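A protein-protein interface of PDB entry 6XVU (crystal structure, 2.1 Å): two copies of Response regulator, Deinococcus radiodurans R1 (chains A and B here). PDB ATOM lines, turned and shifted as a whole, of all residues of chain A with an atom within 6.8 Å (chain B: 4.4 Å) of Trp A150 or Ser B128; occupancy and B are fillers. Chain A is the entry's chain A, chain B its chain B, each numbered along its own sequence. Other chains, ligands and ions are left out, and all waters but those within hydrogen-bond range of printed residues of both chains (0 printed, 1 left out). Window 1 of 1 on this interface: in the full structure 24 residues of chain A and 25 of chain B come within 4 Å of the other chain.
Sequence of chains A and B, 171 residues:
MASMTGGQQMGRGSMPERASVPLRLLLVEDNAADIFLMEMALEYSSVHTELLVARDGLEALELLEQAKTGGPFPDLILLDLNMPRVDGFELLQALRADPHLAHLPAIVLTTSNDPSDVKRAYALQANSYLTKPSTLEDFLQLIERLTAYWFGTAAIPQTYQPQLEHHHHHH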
ATOM      1  N   LEU A  23      -9.523 -11.997 -37.579  1.00  0.00           N
ATOM      2  CA  LEU A  23      -9.446 -11.771 -36.117  1.00  0.00           C
ATOM      3  C   LEU A  23      -7.972 -11.739 -35.745  1.00  0.00           C
ATOM      4  O   LEU A  23      -7.220 -12.578 -36.264  1.00  0.00           O
ATOM      5  CB  LEU A  23     -10.238 -12.863 -35.396  1.00  0.00           C
ATOM      6  CG  LEU A  23     -11.724 -12.771 -35.693  1.00  0.00           C
ATOM      7  CD1 LEU A  23     -12.350 -14.092 -35.357  1.00  0.00           C
ATOM      8  CD2 LEU A  23     -12.391 -11.606 -34.967  1.00  0.00           C
ATOM      9  N   ASP A  75      -8.090  -8.644 -31.009  1.00  0.00           N
ATOM     10  CA  ASP A  75      -9.342  -9.233 -30.491  1.00  0.00           C
ATOM     11  C   ASP A  75      -9.056  -9.988 -29.200  1.00  0.00           C
ATOM     12  O   ASP A  75      -9.952 -10.078 -28.360  1.00  0.00           O
ATOM     13  CB  ASP A  75      -9.957 -10.080 -31.603  1.00  0.00           C
ATOM     14  CG  ASP A  75     -10.283  -9.201 -32.804  1.00  0.00           C
ATOM     15  OD1 ASP A  75     -11.264  -8.459 -32.688  1.00  0.00           O
ATOM     16  OD2 ASP A  75      -9.480  -9.179 -33.794  1.00  0.00           O
ATOM     17  N   LEU A  76      -7.832 -10.510 -29.055  1.00  0.00           N
ATOM     18  CA  LEU A  76      -7.497 -11.438 -27.947  1.00  0.00           C
ATOM     19  C   LEU A  76      -5.990 -11.383 -27.699  1.00  0.00           C
ATOM     20  O   LEU A  76      -5.216 -11.289 -28.730  1.00  0.00           O
ATOM     21  CB  LEU A  76      -7.910 -12.815 -28.460  1.00  0.00           C
ATOM     22  CG  LEU A  76      -8.035 -13.923 -27.445  1.00  0.00           C
ATOM     23  CD1 LEU A  76      -9.265 -13.631 -26.619  1.00  0.00           C
ATOM     24  CD2 LEU A  76      -8.178 -15.277 -28.132  1.00  0.00           C
ATOM     25  N   LEU A  78      -2.928 -13.626 -25.861  1.00  0.00           N
ATOM     26  CA  LEU A  78      -2.468 -14.874 -25.220  1.00  0.00           C
ATOM     27  C   LEU A  78      -1.084 -14.571 -24.654  1.00  0.00           C
ATOM     28  O   LEU A  78      -0.229 -14.103 -25.392  1.00  0.00           O
ATOM     29  CB  LEU A  78      -2.371 -16.014 -26.216  1.00  0.00           C
ATOM     30  CG  LEU A  78      -3.680 -16.540 -26.818  1.00  0.00           C
ATOM     31  CD1 LEU A  78      -3.392 -17.692 -27.755  1.00  0.00           C
ATOM     32  CD2 LEU A  78      -4.604 -17.021 -25.741  1.00  0.00           C
ATOM     33  N   PRO A 105      -9.603  -9.068 -23.815  1.00  0.00           N
ATOM     34  CA  PRO A 105      -9.526 -10.420 -23.272  1.00  0.00           C
ATOM     35  C   PRO A 105      -8.065 -10.889 -23.229  1.00  0.00           C
ATOM     36  O   PRO A 105      -7.376 -10.817 -24.223  1.00  0.00           O
ATOM     37  CB  PRO A 105     -10.364 -11.245 -24.259  1.00  0.00           C
ATOM     38  CG  PRO A 105     -11.237 -10.203 -24.972  1.00  0.00           C
ATOM     39  CD  PRO A 105     -10.362  -8.970 -25.072  1.00  0.00           C
ATOM     40  N   ALA A 106      -7.624 -11.336 -22.057  1.00  0.00           N
ATOM     41  CA  ALA A 106      -6.227 -11.723 -21.821  1.00  0.00           C
ATOM     42  C   ALA A 106      -6.237 -13.113 -21.228  1.00  0.00           C
ATOM     43  O   ALA A 106      -6.811 -13.321 -20.168  1.00  0.00           O
ATOM     44  CB  ALA A 106      -5.576 -10.729 -20.906  1.00  0.00           C
ATOM     45  N   ILE A 107      -5.676 -14.034 -21.966  1.00  0.00           N
ATOM     46  CA  ILE A 107      -5.665 -15.464 -21.591  1.00  0.00           C
ATOM     47  C   ILE A 107      -4.222 -15.880 -21.407  1.00  0.00           C
ATOM     48  O   ILE A 107      -3.391 -15.646 -22.289  1.00  0.00           O
ATOM     49  CB  ILE A 107      -6.375 -16.269 -22.664  1.00  0.00           C
ATOM     50  CG1 ILE A 107      -7.833 -15.833 -22.765  1.00  0.00           C
ATOM     51  CG2 ILE A 107      -6.205 -17.738 -22.444  1.00  0.00           C
ATOM     52  CD1 ILE A 107      -8.304 -16.005 -24.166  1.00  0.00           C
ATOM     53  N   ASN A 127      -8.732 -13.307 -18.175  1.00  0.00           N
ATOM     54  CA  ASN A 127     -10.045 -13.867 -18.572  1.00  0.00           C
ATOM     55  C   ASN A 127     -10.026 -15.374 -18.404  1.00  0.00           C
ATOM     56  O   ASN A 127     -11.034 -15.940 -17.952  1.00  0.00           O
ATOM     57  CB  ASN A 127     -10.366 -13.400 -19.977  1.00  0.00           C
ATOM     58  CG  ASN A 127     -10.615 -11.906 -19.972  1.00  0.00           C
ATOM     59  OD1 ASN A 127      -9.649 -11.133 -19.875  1.00  0.00           O
ATOM     60  ND2 ASN A 127     -11.884 -11.524 -20.109  1.00  0.00           N
ATOM     61  N   SER A 128      -8.895 -16.027 -18.701  1.00  0.00           N
ATOM     62  CA  SER A 128      -8.810 -17.499 -18.649  1.00  0.00           C
ATOM     63  C   SER A 128      -7.351 -17.919 -18.561  1.00  0.00           C
ATOM     64  O   SER A 128      -6.444 -17.059 -18.595  1.00  0.00           O
ATOM     65  CB  SER A 128      -9.574 -18.086 -19.842  1.00  0.00           C
ATOM     66  OG  SER A 128      -9.813 -19.459 -19.691  1.00  0.00           O
ATOM     67  N   LEU A 130      -4.814 -21.376 -19.756  1.00  0.00           N
ATOM     68  CA  LEU A 130      -4.656 -22.635 -20.515  1.00  0.00           C
ATOM     69  C   LEU A 130      -3.221 -23.111 -20.275  1.00  0.00           C
ATOM     70  O   LEU A 130      -2.268 -22.323 -20.365  1.00  0.00           O
ATOM     71  CB  LEU A 130      -4.917 -22.407 -22.005  1.00  0.00           C
ATOM     72  CG  LEU A 130      -6.254 -21.757 -22.360  1.00  0.00           C
ATOM     73  CD1 LEU A 130      -6.233 -21.339 -23.823  1.00  0.00           C
ATOM     74  CD2 LEU A 130      -7.406 -22.684 -22.067  1.00  0.00           C
ATOM     75  N   ARG A 145      -9.812 -25.455 -29.954  1.00  0.00           N
ATOM     76  CA  ARG A 145     -10.873 -25.211 -28.953  1.00  0.00           C
ATOM     77  C   ARG A 145     -10.837 -23.779 -28.425  1.00  0.00           C
ATOM     78  O   ARG A 145     -11.879 -23.207 -28.267  1.00  0.00           O
ATOM     79  CB  ARG A 145     -10.697 -26.239 -27.851  1.00  0.00           C
ATOM     80  CG  ARG A 145     -11.274 -27.582 -28.273  1.00  0.00           C
ATOM     81  CD  ARG A 145     -10.716 -28.523 -27.289  1.00  0.00           C
ATOM     82  NE  ARG A 145     -11.239 -29.873 -27.373  1.00  0.00           N
ATOM     83  CZ  ARG A 145     -10.855 -30.812 -26.530  1.00  0.00           C
ATOM     84  NH1 ARG A 145      -9.989 -30.514 -25.566  1.00  0.00           N
ATOM     85  NH2 ARG A 145     -11.349 -32.023 -26.619  1.00  0.00           N
ATOM     86  N   LEU A 146      -9.650 -23.227 -28.200  1.00  0.00           N
ATOM     87  CA  LEU A 146      -9.466 -21.816 -27.764  1.00  0.00           C
ATOM     88  C   LEU A 146     -10.169 -20.921 -28.801  1.00  0.00           C
ATOM     89  O   LEU A 146     -10.958 -20.061 -28.420  1.00  0.00           O
ATOM     90  CB  LEU A 146      -7.943 -21.628 -27.744  1.00  0.00           C
ATOM     91  CG  LEU A 146      -7.342 -20.305 -27.359  1.00  0.00           C
ATOM     92  CD1 LEU A 146      -5.836 -20.556 -27.189  1.00  0.00           C
ATOM     93  CD2 LEU A 146      -7.618 -19.223 -28.376  1.00  0.00           C
ATOM     94  N   THR A 147      -9.863 -21.131 -30.082  1.00  0.00           N
ATOM     95  CA  THR A 147     -10.357 -20.250 -31.165  1.00  0.00           C
ATOM     96  C   THR A 147     -11.858 -20.496 -31.357  1.00  0.00           C
ATOM     97  O   THR A 147     -12.586 -19.492 -31.471  1.00  0.00           O
ATOM     98  CB  THR A 147      -9.558 -20.387 -32.458  1.00  0.00           C
ATOM     99  OG1 THR A 147      -9.622 -21.758 -32.860  1.00  0.00           O
ATOM    100  CG2 THR A 147      -8.132 -19.909 -32.284  1.00  0.00           C
ATOM    101  N   ALA A 148     -12.334 -21.745 -31.313  1.00  0.00           N
ATOM    102  CA  ALA A 148     -13.792 -22.029 -31.446  1.00  0.00           C
ATOM    103  C   ALA A 148     -14.518 -21.324 -30.294  1.00  0.00           C
ATOM    104  O   ALA A 148     -15.588 -20.785 -30.540  1.00  0.00           O
ATOM    105  CB  ALA A 148     -14.080 -23.520 -31.475  1.00  0.00           C
ATOM    106  N   TYR A 149     -13.958 -21.277 -29.084  1.00  0.00           N
ATOM    107  CA  TYR A 149     -14.666 -20.653 -27.926  1.00  0.00           C
ATOM    108  C   TYR A 149     -14.602 -19.120 -28.048  1.00  0.00           C
ATOM    109  O   TYR A 149     -15.654 -18.456 -28.087  1.00  0.00           O
ATOM    110  CB  TYR A 149     -14.091 -21.121 -26.586  1.00  0.00           C
ATOM    111  CG  TYR A 149     -14.794 -20.448 -25.456  1.00  0.00           C
ATOM    112  CD1 TYR A 149     -16.062 -20.870 -25.059  1.00  0.00           C
ATOM    113  CD2 TYR A 149     -14.267 -19.295 -24.884  1.00  0.00           C
ATOM    114  CE1 TYR A 149     -16.729 -20.244 -24.013  1.00  0.00           C
ATOM    115  CE2 TYR A 149     -14.934 -18.647 -23.862  1.00  0.00           C
ATOM    116  CZ  TYR A 149     -16.180 -19.099 -23.467  1.00  0.00           C
ATOM    117  OH  TYR A 149     -16.830 -18.428 -22.482  1.00  0.00           O
ATOM    118  N   TRP A 150     -13.411 -18.543 -28.077  1.00  0.00           N
ATOM    119  CA  TRP A 150     -13.248 -17.066 -27.994  1.00  0.00           C
ATOM    120  C   TRP A 150     -13.724 -16.381 -29.280  1.00  0.00           C
ATOM    121  O   TRP A 150     -14.184 -15.226 -29.202  1.00  0.00           O
ATOM    122  CB  TRP A 150     -11.790 -16.723 -27.672  1.00  0.00           C
ATOM    123  CG  TRP A 150     -11.510 -17.065 -26.249  1.00  0.00           C
ATOM    124  CD1 TRP A 150     -10.820 -18.149 -25.782  1.00  0.00           C
ATOM    125  CD2 TRP A 150     -12.040 -16.382 -25.096  1.00  0.00           C
ATOM    126  NE1 TRP A 150     -10.864 -18.172 -24.419  1.00  0.00           N
ATOM    127  CE2 TRP A 150     -11.588 -17.088 -23.968  1.00  0.00           C
ATOM    128  CE3 TRP A 150     -12.849 -15.257 -24.919  1.00  0.00           C
ATOM    129  CZ2 TRP A 150     -11.939 -16.716 -22.670  1.00  0.00           C
ATOM    130  CZ3 TRP A 150     -13.133 -14.855 -23.637  1.00  0.00           C
ATOM    131  CH2 TRP A 150     -12.654 -15.558 -22.535  1.00  0.00           C
ATOM    132  N   PHE A 151     -13.619 -17.057 -30.426  1.00  0.00           N
ATOM    133  CA  PHE A 151     -13.951 -16.443 -31.730  1.00  0.00           C
ATOM    134  C   PHE A 151     -15.219 -17.041 -32.343  1.00  0.00           C
ATOM    135  O   PHE A 151     -15.549 -16.646 -33.458  1.00  0.00           O
ATOM    136  CB  PHE A 151     -12.760 -16.601 -32.676  1.00  0.00           C
ATOM    137  CG  PHE A 151     -11.496 -15.854 -32.316  1.00  0.00           C
ATOM    138  CD1 PHE A 151     -11.515 -14.635 -31.648  1.00  0.00           C
ATOM    139  CD2 PHE A 151     -10.280 -16.375 -32.727  1.00  0.00           C
ATOM    140  CE1 PHE A 151     -10.345 -13.948 -31.423  1.00  0.00           C
ATOM    141  CE2 PHE A 151      -9.099 -15.692 -32.484  1.00  0.00           C
ATOM    142  CZ  PHE A 151      -9.133 -14.478 -31.835  1.00  0.00           C
ATOM    143  N   GLY A 152     -15.932 -17.915 -31.645  1.00  0.00           N
ATOM    144  CA  GLY A 152     -17.186 -18.517 -32.158  1.00  0.00           C
ATOM    145  C   GLY A 152     -18.264 -18.492 -31.071  1.00  0.00           C
ATOM    146  O   GLY A 152     -19.252 -17.777 -31.223  1.00  0.00           O
ATOM    147  N   THR A 153     -18.059 -19.196 -29.954  1.00  0.00           N
ATOM    148  CA  THR A 153     -19.099 -19.363 -28.913  1.00  0.00           C
ATOM    149  C   THR A 153     -19.277 -18.038 -28.155  1.00  0.00           C
ATOM    150  O   THR A 153     -20.395 -17.650 -27.914  1.00  0.00           O
ATOM    151  CB  THR A 153     -18.706 -20.513 -27.979  1.00  0.00           C
ATOM    152  OG1 THR A 153     -18.339 -21.602 -28.821  1.00  0.00           O
ATOM    153  CG2 THR A 153     -19.827 -20.910 -27.056  1.00  0.00           C
ATOM    154  N   ALA A 154     -18.180 -17.423 -27.728  1.00  0.00           N
ATOM    155  CA  ALA A 154     -18.199 -16.263 -26.819  1.00  0.00           C
ATOM    156  C   ALA A 154     -18.380 -15.012 -27.662  1.00  0.00           C
ATOM    157  O   ALA A 154     -18.017 -15.021 -28.831  1.00  0.00           O
ATOM    158  CB  ALA A 154     -16.932 -16.210 -25.975  1.00  0.00           C
ATOM    159  N   ALA A 155     -18.884 -13.969 -27.029  1.00  0.00           N
ATOM    160  CA  ALA A 155     -18.810 -12.592 -27.554  1.00  0.00           C
ATOM    161  C   ALA A 155     -17.591 -11.954 -26.883  1.00  0.00           C
ATOM    162  O   ALA A 155     -17.330 -12.217 -25.653  1.00  0.00           O
ATOM    163  CB  ALA A 155     -20.085 -11.848 -27.269  1.00  0.00           C
ATOM    164  N   ILE A 156     -16.819 -11.214 -27.675  1.00  0.00           N
ATOM    165  CA  ILE A 156     -15.647 -10.457 -27.187  1.00  0.00           C
ATOM    166  C   ILE A 156     -15.854  -9.030 -27.675  1.00  0.00           C
ATOM    167  O   ILE A 156     -16.643  -8.814 -28.600  1.00  0.00           O
ATOM    168  CB  ILE A 156     -14.337 -11.083 -27.720  1.00  0.00           C
ATOM    169  CG1 ILE A 156     -14.339 -11.161 -29.255  1.00  0.00           C
ATOM    170  CG2 ILE A 156     -14.127 -12.442 -27.074  1.00  0.00           C
ATOM    171  CD1 ILE A 156     -13.028 -11.614 -29.835  1.00  0.00           C
ATOM    172  N   ALA B 106     -16.276 -15.309 -13.584  1.00  0.00           N
ATOM    173  CA  ALA B 106     -17.612 -14.692 -13.646  1.00  0.00           C
ATOM    174  C   ALA B 106     -17.933 -14.413 -15.098  1.00  0.00           C
ATOM    175  O   ALA B 106     -17.191 -13.701 -15.757  1.00  0.00           O
ATOM    176  CB  ALA B 106     -17.682 -13.469 -12.811  1.00  0.00           C
ATOM    177  N   ILE B 107     -18.966 -15.069 -15.590  1.00  0.00           N
ATOM    178  CA  ILE B 107     -19.398 -15.026 -17.005  1.00  0.00           C
ATOM    179  C   ILE B 107     -20.790 -14.433 -17.086  1.00  0.00           C
ATOM    180  O   ILE B 107     -21.708 -14.859 -16.354  1.00  0.00           O
ATOM    181  CB  ILE B 107     -19.324 -16.432 -17.576  1.00  0.00           C
ATOM    182  CG1 ILE B 107     -17.853 -16.859 -17.600  1.00  0.00           C
ATOM    183  CG2 ILE B 107     -19.963 -16.494 -18.942  1.00  0.00           C
ATOM    184  CD1 ILE B 107     -17.699 -18.313 -17.596  1.00  0.00           C
ATOM    185  N   VAL B 108     -20.900 -13.435 -17.929  1.00  0.00           N
ATOM    186  CA  VAL B 108     -22.183 -12.807 -18.262  1.00  0.00           C
ATOM    187  C   VAL B 108     -22.879 -13.722 -19.269  1.00  0.00           C
ATOM    188  O   VAL B 108     -22.252 -14.151 -20.255  1.00  0.00           O
ATOM    189  CB  VAL B 108     -21.966 -11.397 -18.806  1.00  0.00           C
ATOM    190  CG1 VAL B 108     -23.283 -10.812 -19.274  1.00  0.00           C
ATOM    191  CG2 VAL B 108     -21.330 -10.506 -17.743  1.00  0.00           C
ATOM    192  N   TYR B 122     -16.456  -6.682 -20.074  1.00  0.00           N
ATOM    193  CA  TYR B 122     -15.021  -7.033 -20.139  1.00  0.00           C
ATOM    194  C   TYR B 122     -14.195  -5.979 -19.357  1.00  0.00           C
ATOM    195  O   TYR B 122     -13.217  -6.356 -18.632  1.00  0.00           O
ATOM    196  CB  TYR B 122     -14.576  -7.205 -21.598  1.00  0.00           C
ATOM    197  CG  TYR B 122     -14.851  -8.576 -22.165  1.00  0.00           C
ATOM    198  CD1 TYR B 122     -16.052  -8.868 -22.797  1.00  0.00           C
ATOM    199  CD2 TYR B 122     -13.895  -9.592 -22.096  1.00  0.00           C
ATOM    200  CE1 TYR B 122     -16.320 -10.135 -23.301  1.00  0.00           C
ATOM    201  CE2 TYR B 122     -14.173 -10.873 -22.552  1.00  0.00           C
ATOM    202  CZ  TYR B 122     -15.398 -11.148 -23.156  1.00  0.00           C
ATOM    203  OH  TYR B 122     -15.622 -12.409 -23.630  1.00  0.00           O
ATOM    204  N   ALA B 126     -15.340  -9.084 -16.117  1.00  0.00           N
ATOM    205  CA  ALA B 126     -15.987 -10.382 -16.432  1.00  0.00           C
ATOM    206  C   ALA B 126     -14.956 -11.261 -17.150  1.00  0.00           C
ATOM    207  O   ALA B 126     -14.192 -10.759 -17.947  1.00  0.00           O
ATOM    208  CB  ALA B 126     -17.189 -10.185 -17.296  1.00  0.00           C
ATOM    209  N   ASN B 127     -14.944 -12.544 -16.880  1.00  0.00           N
ATOM    210  CA  ASN B 127     -14.048 -13.483 -17.590  1.00  0.00           C
ATOM    211  C   ASN B 127     -14.539 -13.681 -19.029  1.00  0.00           C
ATOM    212  O   ASN B 127     -13.708 -13.767 -19.909  1.00  0.00           O
ATOM    213  CB  ASN B 127     -13.939 -14.781 -16.809  1.00  0.00           C
ATOM    214  CG  ASN B 127     -13.220 -14.518 -15.513  1.00  0.00           C
ATOM    215  OD1 ASN B 127     -13.855 -13.970 -14.622  1.00  0.00           O
ATOM    216  ND2 ASN B 127     -11.960 -14.929 -15.395  1.00  0.00           N
ATOM    217  N   SER B 128     -15.851 -13.676 -19.259  1.00  0.00           N
ATOM    218  CA  SER B 128     -16.399 -13.896 -20.617  1.00  0.00           C
ATOM    219  C   SER B 128     -17.825 -13.392 -20.683  1.00  0.00           C
ATOM    220  O   SER B 128     -18.395 -12.962 -19.627  1.00  0.00           O
ATOM    221  CB  SER B 128     -16.284 -15.383 -20.972  1.00  0.00           C
ATOM    222  OG  SER B 128     -16.373 -15.609 -22.370  1.00  0.00           O
ATOM    223  N   TYR B 129     -18.367 -13.425 -21.895  1.00  0.00           N
ATOM    224  CA  TYR B 129     -19.726 -12.933 -22.190  1.00  0.00           C
ATOM    225  C   TYR B 129     -20.333 -13.889 -23.193  1.00  0.00           C
ATOM    226  O   TYR B 129     -19.676 -14.143 -24.221  1.00  0.00           O
ATOM    227  CB  TYR B 129     -19.632 -11.533 -22.745  1.00  0.00           C
ATOM    228  CG  TYR B 129     -20.930 -10.762 -22.863  1.00  0.00           C
ATOM    229  CD1 TYR B 129     -21.889 -11.102 -23.815  1.00  0.00           C
ATOM    230  CD2 TYR B 129     -21.128  -9.601 -22.125  1.00  0.00           C
ATOM    231  CE1 TYR B 129     -22.998 -10.305 -24.022  1.00  0.00           C
ATOM    232  CE2 TYR B 129     -22.256  -8.816 -22.305  1.00  0.00           C
ATOM    233  CZ  TYR B 129     -23.195  -9.166 -23.255  1.00  0.00           C
ATOM    234  OH  TYR B 129     -24.296  -8.412 -23.459  1.00  0.00           O
ATOM    235  N   TYR B 149     -15.540 -25.818 -22.255  1.00  0.00           N
ATOM    236  CA  TYR B 149     -14.413 -24.884 -22.229  1.00  0.00           C
ATOM    237  C   TYR B 149     -13.965 -24.659 -20.763  1.00  0.00           C
ATOM    238  O   TYR B 149     -12.770 -24.880 -20.416  1.00  0.00           O
ATOM    239  CB  TYR B 149     -14.733 -23.576 -22.945  1.00  0.00           C
ATOM    240  CG  TYR B 149     -13.583 -22.628 -22.831  1.00  0.00           C
ATOM    241  CD1 TYR B 149     -12.498 -22.772 -23.663  1.00  0.00           C
ATOM    242  CD2 TYR B 149     -13.497 -21.703 -21.792  1.00  0.00           C
ATOM    243  CE1 TYR B 149     -11.394 -21.945 -23.556  1.00  0.00           C
ATOM    244  CE2 TYR B 149     -12.380 -20.910 -21.624  1.00  0.00           C
ATOM    245  CZ  TYR B 149     -11.334 -21.026 -22.520  1.00  0.00           C
ATOM    246  OH  TYR B 149     -10.215 -20.296 -22.387  1.00  0.00           O
ATOM    247  N   TRP B 150     -14.851 -24.168 -19.920  1.00  0.00           N
ATOM    248  CA  TRP B 150     -14.486 -23.722 -18.553  1.00  0.00           C
ATOM    249  C   TRP B 150     -14.145 -24.922 -17.661  1.00  0.00           C
ATOM    250  O   TRP B 150     -13.335 -24.761 -16.755  1.00  0.00           O
ATOM    251  CB  TRP B 150     -15.616 -22.865 -17.972  1.00  0.00           C
ATOM    252  CG  TRP B 150     -15.636 -21.557 -18.683  1.00  0.00           C
ATOM    253  CD1 TRP B 150     -16.490 -21.148 -19.651  1.00  0.00           C
ATOM    254  CD2 TRP B 150     -14.662 -20.513 -18.537  1.00  0.00           C
ATOM    255  NE1 TRP B 150     -16.107 -19.931 -20.144  1.00  0.00           N
ATOM    256  CE2 TRP B 150     -14.998 -19.504 -19.459  1.00  0.00           C
ATOM    257  CE3 TRP B 150     -13.530 -20.356 -17.736  1.00  0.00           C
ATOM    258  CZ2 TRP B 150     -14.216 -18.365 -19.634  1.00  0.00           C
ATOM    259  CZ3 TRP B 150     -12.806 -19.202 -17.849  1.00  0.00           C
ATOM    260  CH2 TRP B 150     -13.151 -18.220 -18.782  1.00  0.00           C
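Hydrophobic or aromatic side chains of chain A that line the printed part of chain B: Pro A105, Leu A130, Tyr A149, Trp A150, Ala A154, Ala A155 and Ile A156.
Hydrophobic or aromatic side chains of chain B within 4 Å of the printed part of chain A: Tyr B122, Tyr B129, Tyr B149 and Trp B150.
Among the printed residues, 20 pairs touch across the chains.
ND2 of Asn A127 lies within hydrogen-bond range of O of Ala B126, 3.3 Å away.
ND2 of Asn A127 is in hydrogen-bond range of O of Asn B127 (2.9 Å).
The side-chain hydroxyl (OG) of Ser A128 is in hydrogen-bond range of the side-chain hydroxyl (OH) of Tyr B149.
The side-chain hydroxyl (OG) of Ser B128 sits at hydrogen-bond distance from the side-chain hydroxyl (OH) of Tyr A149 (2.9 Å).
OH of Tyr A149 sits at hydrogen-bond distance from NE1 of Trp B150.
The side-chain hydroxyl of Tyr B149 is in hydrogen-bond range of the indole nitrogen of Trp A150 (3.0 Å).
O of Ala A155 lies within hydrogen-bond range of OH of Tyr B122, at 2.7 Å.
N of Ala A155 is in hydrogen-bond range of O of Tyr B129, 2.9 Å away.
Of the printed residues of chain B, Pro A105 touches Tyr B122.
Printed residues of chain B within 4 Å of Asn A127: Tyr B122 (3.4 Å), Ala B126 (3.3 Å), Asn B127 (2.9 Å) and Trp B150 (3.2 Å).
Thr A147 touches none of the printed residues of chain B.
Printed residues of chain B within 4 Å of Trp A150: Tyr B122 (3.5 Å), Asn B127 (3.3 Å), Ser B128 (3.6 Å) and Tyr B149 (3.0 Å).
Of the printed residues of chain B, Ala A155 touches Tyr B122 and Tyr B129.
Printed residues of chain B within 4 Å of Ile A156: Tyr B122.
Ala B106 touches none of the printed residues of chain A.
Of chain A, only Tyr A149, Trp A150 and Ala A154 come within 4 Å of Ser B128.
Printed residues of chain A within 4 Å of Tyr B149: Ser A128, Leu A130, Tyr A149 and Trp A150.
The nearest residue of chain A that does not touch Ser B128 is Asn A127 (4.6 Å).
The nearest printed residue of chain A that does not touch Trp B150 is Trp A150 (4.1 Å).
Asn B127 touches its own counterpart, Asn A127.
Ser A128 touches Tyr B149, and with the chains exchanged Tyr A149 touches Ser B128.
Ser A128 touches Trp B150, and with the chains exchanged Trp A150 touches Ser B128.
Tyr A149 touches Trp B150, and with the chains exchanged Trp A150 touches Tyr B149.
Positions printed for both chains: 106, 107, 127, 128, 149 and 150.
The backbone carbonyl oxygen (O) of Ala A106 is in hydrogen-bond range of the backbone NH (N) of Asn A127 (2.8 Å).
N of Ala A154 lies within hydrogen-bond range of O of Tyr A149.
N of Asn B127 lies within hydrogen-bond range of O of Ala B106 (2.8 Å).
N of Val B108 lies within hydrogen-bond range of O of Ser B128.
The side-chain hydroxyl (OH) of Tyr B122 sits at hydrogen-bond distance from the backbone NH (N) of Tyr B129 (3.4 Å).
Among the printed residues, pairs that only touch across the chains: Pro A105 with Tyr B122 (3.9 Å), Asn A127 with Tyr B122 (3.4 Å), Asn A127 with Trp B150 (3.2 Å), Ser A128 with Trp B150 (3.5 Å), Leu A130 with Tyr B149 (3.7 Å), Tyr A149 with Tyr B149 (3.6 Å), Trp A150 with Tyr B122 (3.5 Å), Trp A150 with Asn B127 (3.3 Å), Trp A150 with Ser B128 (3.6 Å), Ala A154 with Ser B128 (3.7 Å), Ala A154 with Tyr B129 (3.7 Å) and Ile A156 with Tyr B122 (3.8 Å).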
